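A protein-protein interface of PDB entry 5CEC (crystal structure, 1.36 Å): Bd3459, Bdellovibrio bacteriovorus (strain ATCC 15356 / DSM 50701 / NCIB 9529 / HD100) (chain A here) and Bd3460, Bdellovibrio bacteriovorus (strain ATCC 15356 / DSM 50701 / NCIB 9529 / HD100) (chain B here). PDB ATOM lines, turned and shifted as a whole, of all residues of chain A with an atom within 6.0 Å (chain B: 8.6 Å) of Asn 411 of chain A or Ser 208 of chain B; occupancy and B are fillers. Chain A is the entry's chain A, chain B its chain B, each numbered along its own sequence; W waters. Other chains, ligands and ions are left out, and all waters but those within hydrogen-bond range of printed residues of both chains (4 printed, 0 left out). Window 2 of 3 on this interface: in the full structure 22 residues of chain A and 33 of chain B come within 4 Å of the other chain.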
ATOM      1  N   VAL A 349      -8.768  22.569 -29.645  1.00  0.00           N
ATOM      2  CA  VAL A 349      -9.472  21.727 -28.680  1.00  0.00           C
ATOM      3  C   VAL A 349      -9.872  20.356 -29.228  1.00  0.00           C
ATOM      4  O   VAL A 349     -10.158  19.454 -28.445  1.00  0.00           O
ATOM      5  CB  VAL A 349     -10.689  22.428 -28.088  1.00  0.00           C
ATOM      6  CG1 VAL A 349     -10.242  23.620 -27.259  1.00  0.00           C
ATOM      7  CG2 VAL A 349     -11.725  22.827 -29.132  1.00  0.00           C
ATOM      8  N   VAL A 406     -17.068  22.912 -34.539  1.00  0.00           N
ATOM      9  CA  VAL A 406     -16.869  21.790 -33.615  1.00  0.00           C
ATOM     10  C   VAL A 406     -16.134  22.269 -32.357  1.00  0.00           C
ATOM     11  O   VAL A 406     -16.473  21.859 -31.236  1.00  0.00           O
ATOM     12  CB  VAL A 406     -16.143  20.620 -34.303  1.00  0.00           C
ATOM     13  CG1 VAL A 406     -15.872  19.489 -33.311  1.00  0.00           C
ATOM     14  CG2 VAL A 406     -16.987  20.152 -35.475  1.00  0.00           C
ATOM     15  N   SER A 407     -15.171  23.172 -32.520  1.00  0.00           N
ATOM     16  CA  SER A 407     -14.441  23.702 -31.368  1.00  0.00           C
ATOM     17  C   SER A 407     -15.392  24.459 -30.439  1.00  0.00           C
ATOM     18  O   SER A 407     -15.309  24.349 -29.205  1.00  0.00           O
ATOM     19  CB  SER A 407     -13.306  24.604 -31.829  1.00  0.00           C
ATOM     20  OG  SER A 407     -12.384  23.872 -32.592  1.00  0.00           O
ATOM     21  N   GLN A 408     -16.319  25.213 -31.024  1.00  0.00           N
ATOM     22  CA  GLN A 408     -17.323  25.955 -30.241  1.00  0.00           C
ATOM     23  C   GLN A 408     -18.173  24.976 -29.437  1.00  0.00           C
ATOM     24  O   GLN A 408     -18.454  25.230 -28.250  1.00  0.00           O
ATOM     25  CB  GLN A 408     -18.199  26.809 -31.166  1.00  0.00           C
ATOM     26  CG  GLN A 408     -19.186  27.727 -30.454  1.00  0.00           C
ATOM     27  CD  GLN A 408     -18.500  28.750 -29.552  1.00  0.00           C
ATOM     28  OE1 GLN A 408     -17.478  29.333 -29.898  1.00  0.00           O
ATOM     29  NE2 GLN A 408     -19.061  28.959 -28.384  1.00  0.00           N
ATOM     30  N   LEU A 409     -18.596  23.879 -30.075  1.00  0.00           N
ATOM     31  CA  LEU A 409     -19.363  22.851 -29.374  1.00  0.00           C
ATOM     32  C   LEU A 409     -18.614  22.289 -28.163  1.00  0.00           C
ATOM     33  O   LEU A 409     -19.183  22.101 -27.069  1.00  0.00           O
ATOM     34  CB  LEU A 409     -19.788  21.735 -30.349  1.00  0.00           C
ATOM     35  CG  LEU A 409     -20.536  20.547 -29.745  1.00  0.00           C
ATOM     36  CD1 LEU A 409     -21.884  20.969 -29.158  1.00  0.00           C
ATOM     37  CD2 LEU A 409     -20.740  19.475 -30.799  1.00  0.00           C
ATOM     38  N   ILE A 410     -17.327  22.055 -28.344  1.00  0.00           N
ATOM     39  CA  ILE A 410     -16.489  21.596 -27.239  1.00  0.00           C
ATOM     40  C   ILE A 410     -16.390  22.653 -26.117  1.00  0.00           C
ATOM     41  O   ILE A 410     -16.532  22.309 -24.936  1.00  0.00           O
ATOM     42  CB  ILE A 410     -15.071  21.197 -27.766  1.00  0.00           C
ATOM     43  CG1 ILE A 410     -15.164  19.920 -28.592  1.00  0.00           C
ATOM     44  CG2 ILE A 410     -14.114  20.983 -26.591  1.00  0.00           C
ATOM     45  CD1 ILE A 410     -13.927  19.641 -29.407  1.00  0.00           C
ATOM     46  N   ASN A 411     -16.176  23.916 -26.498  1.00  0.00           N
ATOM     47  CA  ASN A 411     -16.090  25.047 -25.564  1.00  0.00           C
ATOM     48  C   ASN A 411     -17.321  25.085 -24.674  1.00  0.00           C
ATOM     49  O   ASN A 411     -17.228  25.299 -23.454  1.00  0.00           O
ATOM     50  CB  ASN A 411     -16.054  26.432 -26.297  1.00  0.00           C
ATOM     51  CG  ASN A 411     -14.740  26.749 -26.992  1.00  0.00           C
ATOM     52  OD1 ASN A 411     -13.699  26.119 -26.758  1.00  0.00           O
ATOM     53  ND2 ASN A 411     -14.790  27.784 -27.885  1.00  0.00           N
ATOM     54  N   GLN A 412     -18.486  24.885 -25.295  1.00  0.00           N
ATOM     55  CA  GLN A 412     -19.771  24.982 -24.606  1.00  0.00           C
ATOM     56  C   GLN A 412     -20.099  23.781 -23.739  1.00  0.00           C
ATOM     57  O   GLN A 412     -21.081  23.809 -22.984  1.00  0.00           O
ATOM     58  CB  GLN A 412     -20.881  25.233 -25.613  1.00  0.00           C
ATOM     59  CG  GLN A 412     -20.746  26.611 -26.214  1.00  0.00           C
ATOM     60  CD  GLN A 412     -21.699  26.862 -27.353  1.00  0.00           C
ATOM     61  OE1 GLN A 412     -22.216  25.932 -27.967  1.00  0.00           O
ATOM     62  NE2 GLN A 412     -21.939  28.121 -27.642  1.00  0.00           N
ATOM     63  N   ASN A 413     -19.234  22.765 -23.779  1.00  0.00           N
ATOM     64  CA  ASN A 413     -19.372  21.586 -22.903  1.00  0.00           C
ATOM     65  C   ASN A 413     -18.149  21.405 -21.986  1.00  0.00           C
ATOM     66  O   ASN A 413     -17.760  20.266 -21.658  1.00  0.00           O
ATOM     67  CB  ASN A 413     -19.609  20.373 -23.811  1.00  0.00           C
ATOM     68  CG  ASN A 413     -21.023  20.338 -24.313  1.00  0.00           C
ATOM     69  OD1 ASN A 413     -21.907  19.911 -23.590  1.00  0.00           O
ATOM     70  ND2 ASN A 413     -21.259  20.836 -25.515  1.00  0.00           N
ATOM     71  N   GLY A 414     -17.556  22.545 -21.583  1.00  0.00           N
ATOM     72  CA  GLY A 414     -16.441  22.590 -20.627  1.00  0.00           C
ATOM     73  C   GLY A 414     -15.052  22.299 -21.101  1.00  0.00           C
ATOM     74  O   GLY A 414     -14.137  22.141 -20.273  1.00  0.00           O
ATOM     75  N   GLY A 415     -14.870  22.303 -22.424  1.00  0.00           N
ATOM     76  CA  GLY A 415     -13.576  22.061 -23.024  1.00  0.00           C
ATOM     77  C   GLY A 415     -13.319  20.589 -23.262  1.00  0.00           C
ATOM     78  O   GLY A 415     -14.138  19.736 -22.880  1.00  0.00           O
ATOM     79  N   ALA B 170      -7.347  33.594 -32.911  1.00  0.00           N
ATOM     80  CA  ALA B 170      -7.953  32.346 -33.369  1.00  0.00           C
ATOM     81  C   ALA B 170      -7.861  31.247 -32.328  1.00  0.00           C
ATOM     82  O   ALA B 170      -8.818  30.533 -32.075  1.00  0.00           O
ATOM     83  CB  ALA B 170      -7.294  31.899 -34.664  1.00  0.00           C
ATOM     84  N   VAL B 171      -6.681  31.113 -31.729  1.00  0.00           N
ATOM     85  CA  VAL B 171      -6.463  30.136 -30.681  1.00  0.00           C
ATOM     86  C   VAL B 171      -7.187  30.520 -29.408  1.00  0.00           C
ATOM     87  O   VAL B 171      -7.666  29.643 -28.670  1.00  0.00           O
ATOM     88  CB  VAL B 171      -4.962  29.899 -30.463  1.00  0.00           C
ATOM     89  CG1 VAL B 171      -4.662  29.131 -29.209  1.00  0.00           C
ATOM     90  CG2 VAL B 171      -4.349  29.294 -31.720  1.00  0.00           C
ATOM     91  N   ALA B 172      -7.304  31.806 -29.133  1.00  0.00           N
ATOM     92  CA  ALA B 172      -8.116  32.246 -27.988  1.00  0.00           C
ATOM     93  C   ALA B 172      -9.534  31.715 -28.126  1.00  0.00           C
ATOM     94  O   ALA B 172     -10.129  31.276 -27.140  1.00  0.00           O
ATOM     95  CB  ALA B 172      -8.115  33.765 -27.888  1.00  0.00           C
ATOM     96  N   ARG B 173     -10.115  31.797 -29.335  1.00  0.00           N
ATOM     97  CA  ARG B 173     -11.482  31.258 -29.503  1.00  0.00           C
ATOM     98  C   ARG B 173     -11.531  29.736 -29.459  1.00  0.00           C
ATOM     99  O   ARG B 173     -12.364  29.156 -28.743  1.00  0.00           O
ATOM    100  CB  ARG B 173     -12.055  31.692 -30.830  1.00  0.00           C
ATOM    101  CG  ARG B 173     -12.346  33.153 -30.943  1.00  0.00           C
ATOM    102  CD  ARG B 173     -13.276  33.428 -32.108  1.00  0.00           C
ATOM    103  NE  ARG B 173     -13.526  34.850 -32.289  1.00  0.00           N
ATOM    104  CZ  ARG B 173     -12.751  35.694 -32.960  1.00  0.00           C
ATOM    105  NH1 ARG B 173     -11.618  35.289 -33.530  1.00  0.00           N
ATOM    106  NH2 ARG B 173     -13.116  36.956 -33.015  1.00  0.00           N
ATOM    107  N   TYR B 174     -10.651  29.087 -30.228  1.00  0.00           N
ATOM    108  CA  TYR B 174     -10.879  27.695 -30.564  1.00  0.00           C
ATOM    109  C   TYR B 174      -9.738  26.742 -30.218  1.00  0.00           C
ATOM    110  O   TYR B 174      -9.788  25.549 -30.570  1.00  0.00           O
ATOM    111  CB  TYR B 174     -11.205  27.595 -32.044  1.00  0.00           C
ATOM    112  CG  TYR B 174     -12.359  28.479 -32.476  1.00  0.00           C
ATOM    113  CD1 TYR B 174     -13.611  28.351 -31.855  1.00  0.00           C
ATOM    114  CD2 TYR B 174     -12.218  29.444 -33.450  1.00  0.00           C
ATOM    115  CE1 TYR B 174     -14.677  29.142 -32.217  1.00  0.00           C
ATOM    116  CE2 TYR B 174     -13.303  30.223 -33.848  1.00  0.00           C
ATOM    117  CZ  TYR B 174     -14.518  30.085 -33.202  1.00  0.00           C
ATOM    118  OH  TYR B 174     -15.573  30.857 -33.554  1.00  0.00           O
ATOM    119  N   GLY B 175      -8.719  27.242 -29.518  1.00  0.00           N
ATOM    120  CA  GLY B 175      -7.554  26.461 -29.169  1.00  0.00           C
ATOM    121  C   GLY B 175      -7.410  26.242 -27.690  1.00  0.00           C
ATOM    122  O   GLY B 175      -8.366  26.379 -26.911  1.00  0.00           O
ATOM    123  N   THR B 176      -6.204  25.845 -27.321  1.00  0.00           N
ATOM    124  CA  THR B 176      -5.896  25.415 -25.976  1.00  0.00           C
ATOM    125  C   THR B 176      -4.887  26.322 -25.298  1.00  0.00           C
ATOM    126  O   THR B 176      -4.210  27.109 -25.958  1.00  0.00           O
ATOM    127  CB  THR B 176      -5.250  24.039 -26.000  1.00  0.00           C
ATOM    128  OG1 THR B 176      -3.999  24.121 -26.688  1.00  0.00           O
ATOM    129  CG2 THR B 176      -6.144  22.978 -26.663  1.00  0.00           C
ATOM    130  N   LEU B 201      -8.136  38.091 -25.179  1.00  0.00           N
ATOM    131  CA  LEU B 201      -8.910  37.704 -24.005  1.00  0.00           C
ATOM    132  C   LEU B 201     -10.408  37.981 -24.235  1.00  0.00           C
ATOM    133  O   LEU B 201     -11.248  37.135 -23.921  1.00  0.00           O
ATOM    134  CB  LEU B 201      -8.412  38.479 -22.775  1.00  0.00           C
ATOM    135  CG  LEU B 201      -9.213  38.274 -21.484  1.00  0.00           C
ATOM    136  CD1 LEU B 201      -9.338  36.796 -21.143  1.00  0.00           C
ATOM    137  CD2 LEU B 201      -8.553  39.029 -20.351  1.00  0.00           C
ATOM    138  N   ASP B 202     -10.734  39.153 -24.791  1.00  0.00           N
ATOM    139  CA  ASP B 202     -12.124  39.501 -25.066  1.00  0.00           C
ATOM    140  C   ASP B 202     -12.758  38.405 -25.954  1.00  0.00           C
ATOM    141  O   ASP B 202     -13.895  37.982 -25.719  1.00  0.00           O
ATOM    142  CB  ASP B 202     -12.251  40.843 -25.787  1.00  0.00           C
ATOM    143  CG  ASP B 202     -11.989  42.030 -24.898  1.00  0.00           C
ATOM    144  OD1 ASP B 202     -12.162  41.951 -23.660  1.00  0.00           O
ATOM    145  OD2 ASP B 202     -11.655  43.077 -25.473  1.00  0.00           O
ATOM    146  N   VAL B 203     -12.057  37.969 -26.993  1.00  0.00           N
ATOM    147  CA  VAL B 203     -12.676  37.011 -27.915  1.00  0.00           C
ATOM    148  C   VAL B 203     -12.749  35.614 -27.320  1.00  0.00           C
ATOM    149  O   VAL B 203     -13.641  34.843 -27.650  1.00  0.00           O
ATOM    150  CB  VAL B 203     -12.074  37.030 -29.348  1.00  0.00           C
ATOM    151  CG1 VAL B 203     -12.069  38.441 -29.899  1.00  0.00           C
ATOM    152  CG2 VAL B 203     -10.703  36.397 -29.425  1.00  0.00           C
ATOM    153  N   ALA B 204     -11.790  35.255 -26.453  1.00  0.00           N
ATOM    154  CA  ALA B 204     -11.914  34.007 -25.707  1.00  0.00           C
ATOM    155  C   ALA B 204     -13.190  33.958 -24.868  1.00  0.00           C
ATOM    156  O   ALA B 204     -13.896  32.972 -24.877  1.00  0.00           O
ATOM    157  CB  ALA B 204     -10.717  33.785 -24.821  1.00  0.00           C
ATOM    158  N   LYS B 205     -13.426  35.025 -24.131  1.00  0.00           N
ATOM    159  CA  LYS B 205     -14.621  35.112 -23.312  1.00  0.00           C
ATOM    160  C   LYS B 205     -15.878  35.024 -24.163  1.00  0.00           C
ATOM    161  O   LYS B 205     -16.792  34.286 -23.854  1.00  0.00           O
ATOM    162  CB  LYS B 205     -14.651  36.424 -22.550  1.00  0.00           C
ATOM    163  CG  LYS B 205     -13.581  36.626 -21.514  1.00  0.00           C
ATOM    164  CD  LYS B 205     -13.818  37.987 -20.880  1.00  0.00           C
ATOM    165  CE  LYS B 205     -12.768  38.364 -19.888  1.00  0.00           C
ATOM    166  NZ  LYS B 205     -12.992  39.797 -19.524  1.00  0.00           N
ATOM    167  N   GLU B 206     -15.889  35.746 -25.264  1.00  0.00           N
ATOM    168  CA  GLU B 206     -17.033  35.755 -26.161  1.00  0.00           C
ATOM    169  C   GLU B 206     -17.335  34.375 -26.775  1.00  0.00           C
ATOM    170  O   GLU B 206     -18.505  34.019 -26.940  1.00  0.00           O
ATOM    171  CB  GLU B 206     -16.799  36.809 -27.244  1.00  0.00           C
ATOM    172  CG  GLU B 206     -17.914  36.944 -28.263  1.00  0.00           C
ATOM    173  CD  GLU B 206     -17.607  37.962 -29.343  1.00  0.00           C
ATOM    174  OE1 GLU B 206     -16.526  37.895 -29.922  1.00  0.00           O
ATOM    175  OE2 GLU B 206     -18.437  38.839 -29.646  1.00  0.00           O
ATOM    176  N   ALA B 207     -16.301  33.591 -27.063  1.00  0.00           N
ATOM    177  CA  ALA B 207     -16.438  32.239 -27.613  1.00  0.00           C
ATOM    178  C   ALA B 207     -16.634  31.162 -26.524  1.00  0.00           C
ATOM    179  O   ALA B 207     -16.672  29.958 -26.841  1.00  0.00           O
ATOM    180  CB  ALA B 207     -15.206  31.908 -28.437  1.00  0.00           C
ATOM    181  N   SER B 208     -16.726  31.584 -25.255  1.00  0.00           N
ATOM    182  CA  SER B 208     -16.963  30.678 -24.117  1.00  0.00           C
ATOM    183  C   SER B 208     -15.840  29.651 -23.966  1.00  0.00           C
ATOM    184  O   SER B 208     -16.069  28.528 -23.545  1.00  0.00           O
ATOM    185  CB  SER B 208     -18.344  30.009 -24.211  1.00  0.00           C
ATOM    186  OG  SER B 208     -19.375  30.999 -24.249  1.00  0.00           O
ATOM    187  N   ASN B 209     -14.614  30.056 -24.307  1.00  0.00           N
ATOM    188  CA  ASN B 209     -13.444  29.223 -24.091  1.00  0.00           C
ATOM    189  C   ASN B 209     -12.888  29.500 -22.747  1.00  0.00           C
ATOM    190  O   ASN B 209     -12.085  30.405 -22.580  1.00  0.00           O
ATOM    191  CB  ASN B 209     -12.400  29.446 -25.186  1.00  0.00           C
ATOM    192  CG  ASN B 209     -11.358  28.353 -25.221  1.00  0.00           C
ATOM    193  OD1 ASN B 209     -10.949  27.814 -24.170  1.00  0.00           O
ATOM    194  ND2 ASN B 209     -10.848  28.071 -26.410  1.00  0.00           N
ATOM    195  N   GLN B 210     -13.393  28.777 -21.744  1.00  0.00           N
ATOM    196  CA  GLN B 210     -13.000  29.033 -20.367  1.00  0.00           C
ATOM    197  C   GLN B 210     -11.500  28.864 -20.185  1.00  0.00           C
ATOM    198  O   GLN B 210     -10.862  29.676 -19.519  1.00  0.00           O
ATOM    199  CB  GLN B 210     -13.731  28.062 -19.409  1.00  0.00           C
ATOM    200  CG  GLN B 210     -15.171  28.404 -19.098  1.00  0.00           C
ATOM    201  CD  GLN B 210     -15.359  29.585 -18.146  1.00  0.00           C
ATOM    202  OE1 GLN B 210     -16.378  30.256 -18.221  1.00  0.00           O
ATOM    203  NE2 GLN B 210     -14.412  29.804 -17.215  1.00  0.00           N
ATOM    204  N   ASP B 211     -10.920  27.822 -20.781  1.00  0.00           N
ATOM    205  CA  ASP B 211      -9.512  27.541 -20.510  1.00  0.00           C
ATOM    206  C   ASP B 211      -8.565  28.588 -21.105  1.00  0.00           C
ATOM    207  O   ASP B 211      -7.610  28.967 -20.448  1.00  0.00           O
ATOM    208  CB  ASP B 211      -9.124  26.150 -21.007  1.00  0.00           C
ATOM    209  CG  ASP B 211      -9.821  25.040 -20.270  1.00  0.00           C
ATOM    210  OD1 ASP B 211     -10.112  25.205 -19.080  1.00  0.00           O
ATOM    211  OD2 ASP B 211     -10.090  23.993 -20.899  1.00  0.00           O
ATOM    212  N   THR B 212      -8.803  29.036 -22.341  1.00  0.00           N
ATOM    213  CA  THR B 212      -7.955  30.074 -22.891  1.00  0.00           C
ATOM    214  C   THR B 212      -8.219  31.441 -22.246  1.00  0.00           C
ATOM    215  O   THR B 212      -7.277  32.225 -22.084  1.00  0.00           O
ATOM    216  CB  THR B 212      -8.089  30.232 -24.410  1.00  0.00           C
ATOM    217  OG1 THR B 212      -9.446  30.526 -24.705  1.00  0.00           O
ATOM    218  CG2 THR B 212      -7.594  28.983 -25.165  1.00  0.00           C
ATOM    219  N   ALA B 213      -9.464  31.714 -21.837  1.00  0.00           N
ATOM    220  CA  ALA B 213      -9.754  32.998 -21.203  1.00  0.00           C
ATOM    221  C   ALA B 213      -9.002  33.071 -19.878  1.00  0.00           C
ATOM    222  O   ALA B 213      -8.359  34.081 -19.574  1.00  0.00           O
ATOM    223  CB  ALA B 213     -11.252  33.206 -20.989  1.00  0.00           C
HETATM  224  O   HOH W   1     -14.953  26.064 -21.745  1.00  0.00           O
HETATM  225  O   HOH W   2     -17.994  27.530 -21.691  1.00  0.00           O
HETATM  226  O   HOH W   3     -17.489  31.353 -31.502  1.00  0.00           O
HETATM  227  O   HOH W   4     -19.988  31.613 -26.876  1.00  0.00           O
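Water W3 lies within hydrogen-bond range of OE1 of Gln 408 of chain A (2.6 Å) and OH of Tyr 174 of chain B (2.9 Å).
Water W4 lies within hydrogen-bond range of OG of Ser 208 of chain B, O of Glu 206 of chain B and NE2 of Gln 408 of chain A.
Water W2 bridges the backbone carbonyl oxygen of Ser 208 of chain B and the backbone carbonyl oxygen of Asn 411 of chain A.
Water W1 lies within hydrogen-bond range of O of Asn 411 of chain A, N of Gln 210 of chain B and O of Ser 208 of chain B.
Of the printed residues of chain B, Ser 407 of chain A touches Tyr 174.
Of chain B, only Arg 173, Ala 207, Ser 208 and Asn 209 come within 4 Å of Asn 411 of chain A.
Gly 414 of chain A touches none of the printed residues of chain B.
Of the printed residues of chain A, Arg 173 of chain B touches Asn 411.
Of the printed residues of chain A, Tyr 174 of chain B touches Val 349 (3.3 Å), Ser 407 (3.7 Å) and Gln 408 (3.6 Å).
Printed residues of chain A within 4 Å of Ala 207 of chain B: Gln 408 and Asn 411.
Ser 208 of chain B touches one residue of chain A.
O of Arg 173 of chain B is in hydrogen-bond range of ND2 of Asn 209 of chain B.
NE2 of Gln 408 of chain A lies close to NE2 of Gln 412 of chain A (3.1 Å).
O of Ala 172 of chain B lies within hydrogen-bond range of ND2 of Asn 209 of chain B (3.4 Å).
The backbone carbonyl oxygen (O) of Gly 175 of chain B lies within hydrogen-bond range of the side-chain amide nitrogen (ND2) of Asn 209 of chain B (3.0 Å).
The side-chain amide oxygen (OD1) of Asn 209 of chain B sits at hydrogen-bond distance from the backbone NH (N) of Thr 212 of chain B, at 3.1 Å.
OD1 of Asn 209 of chain B sits close to N of Asp 211 of chain B (3.4 Å).
Among the printed residues, merely in contact across the chains: Val 349 of chain A with Gly 175 of chain B, Val 349 of chain A with Thr 176 of chain B, Ser 407 of chain A with Tyr 174 of chain B and Gln 408 of chain A with Tyr 174 of chain B.
The side-chain amide nitrogen (ND2) of Asn 411 of chain A sits at hydrogen-bond distance from the backbone carbonyl oxygen (O) of Ala 207 of chain B (3.1 Å).
O of Tyr 174 of chain B sits at hydrogen-bond distance from N of Val 349 of chain A (3.3 Å).
The backbone carbonyl oxygen (O) of Arg 173 of chain B lies within hydrogen-bond range of the side-chain amide nitrogen (ND2) of Asn 411 of chain A (2.9 Å).
NE2 of Gln 408 of chain A lies within hydrogen-bond range of O of Ala 207 of chain B, 3.0 Å away.
The side-chain amide oxygen of Asn 411 of chain A lies within hydrogen-bond range of the side-chain amide nitrogen of Asn 209 of chain B (3.5 Å).
O of Asn 411 of chain A sits close to O of Ser 208 of chain B, 3.4 Å away.
Of the 20 printed residues of chain B, 7 touch a printed residue of chain A.
Hydrophobic or aromatic side chains of chain A within 4 Å of the printed part of chain B: Val 349.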
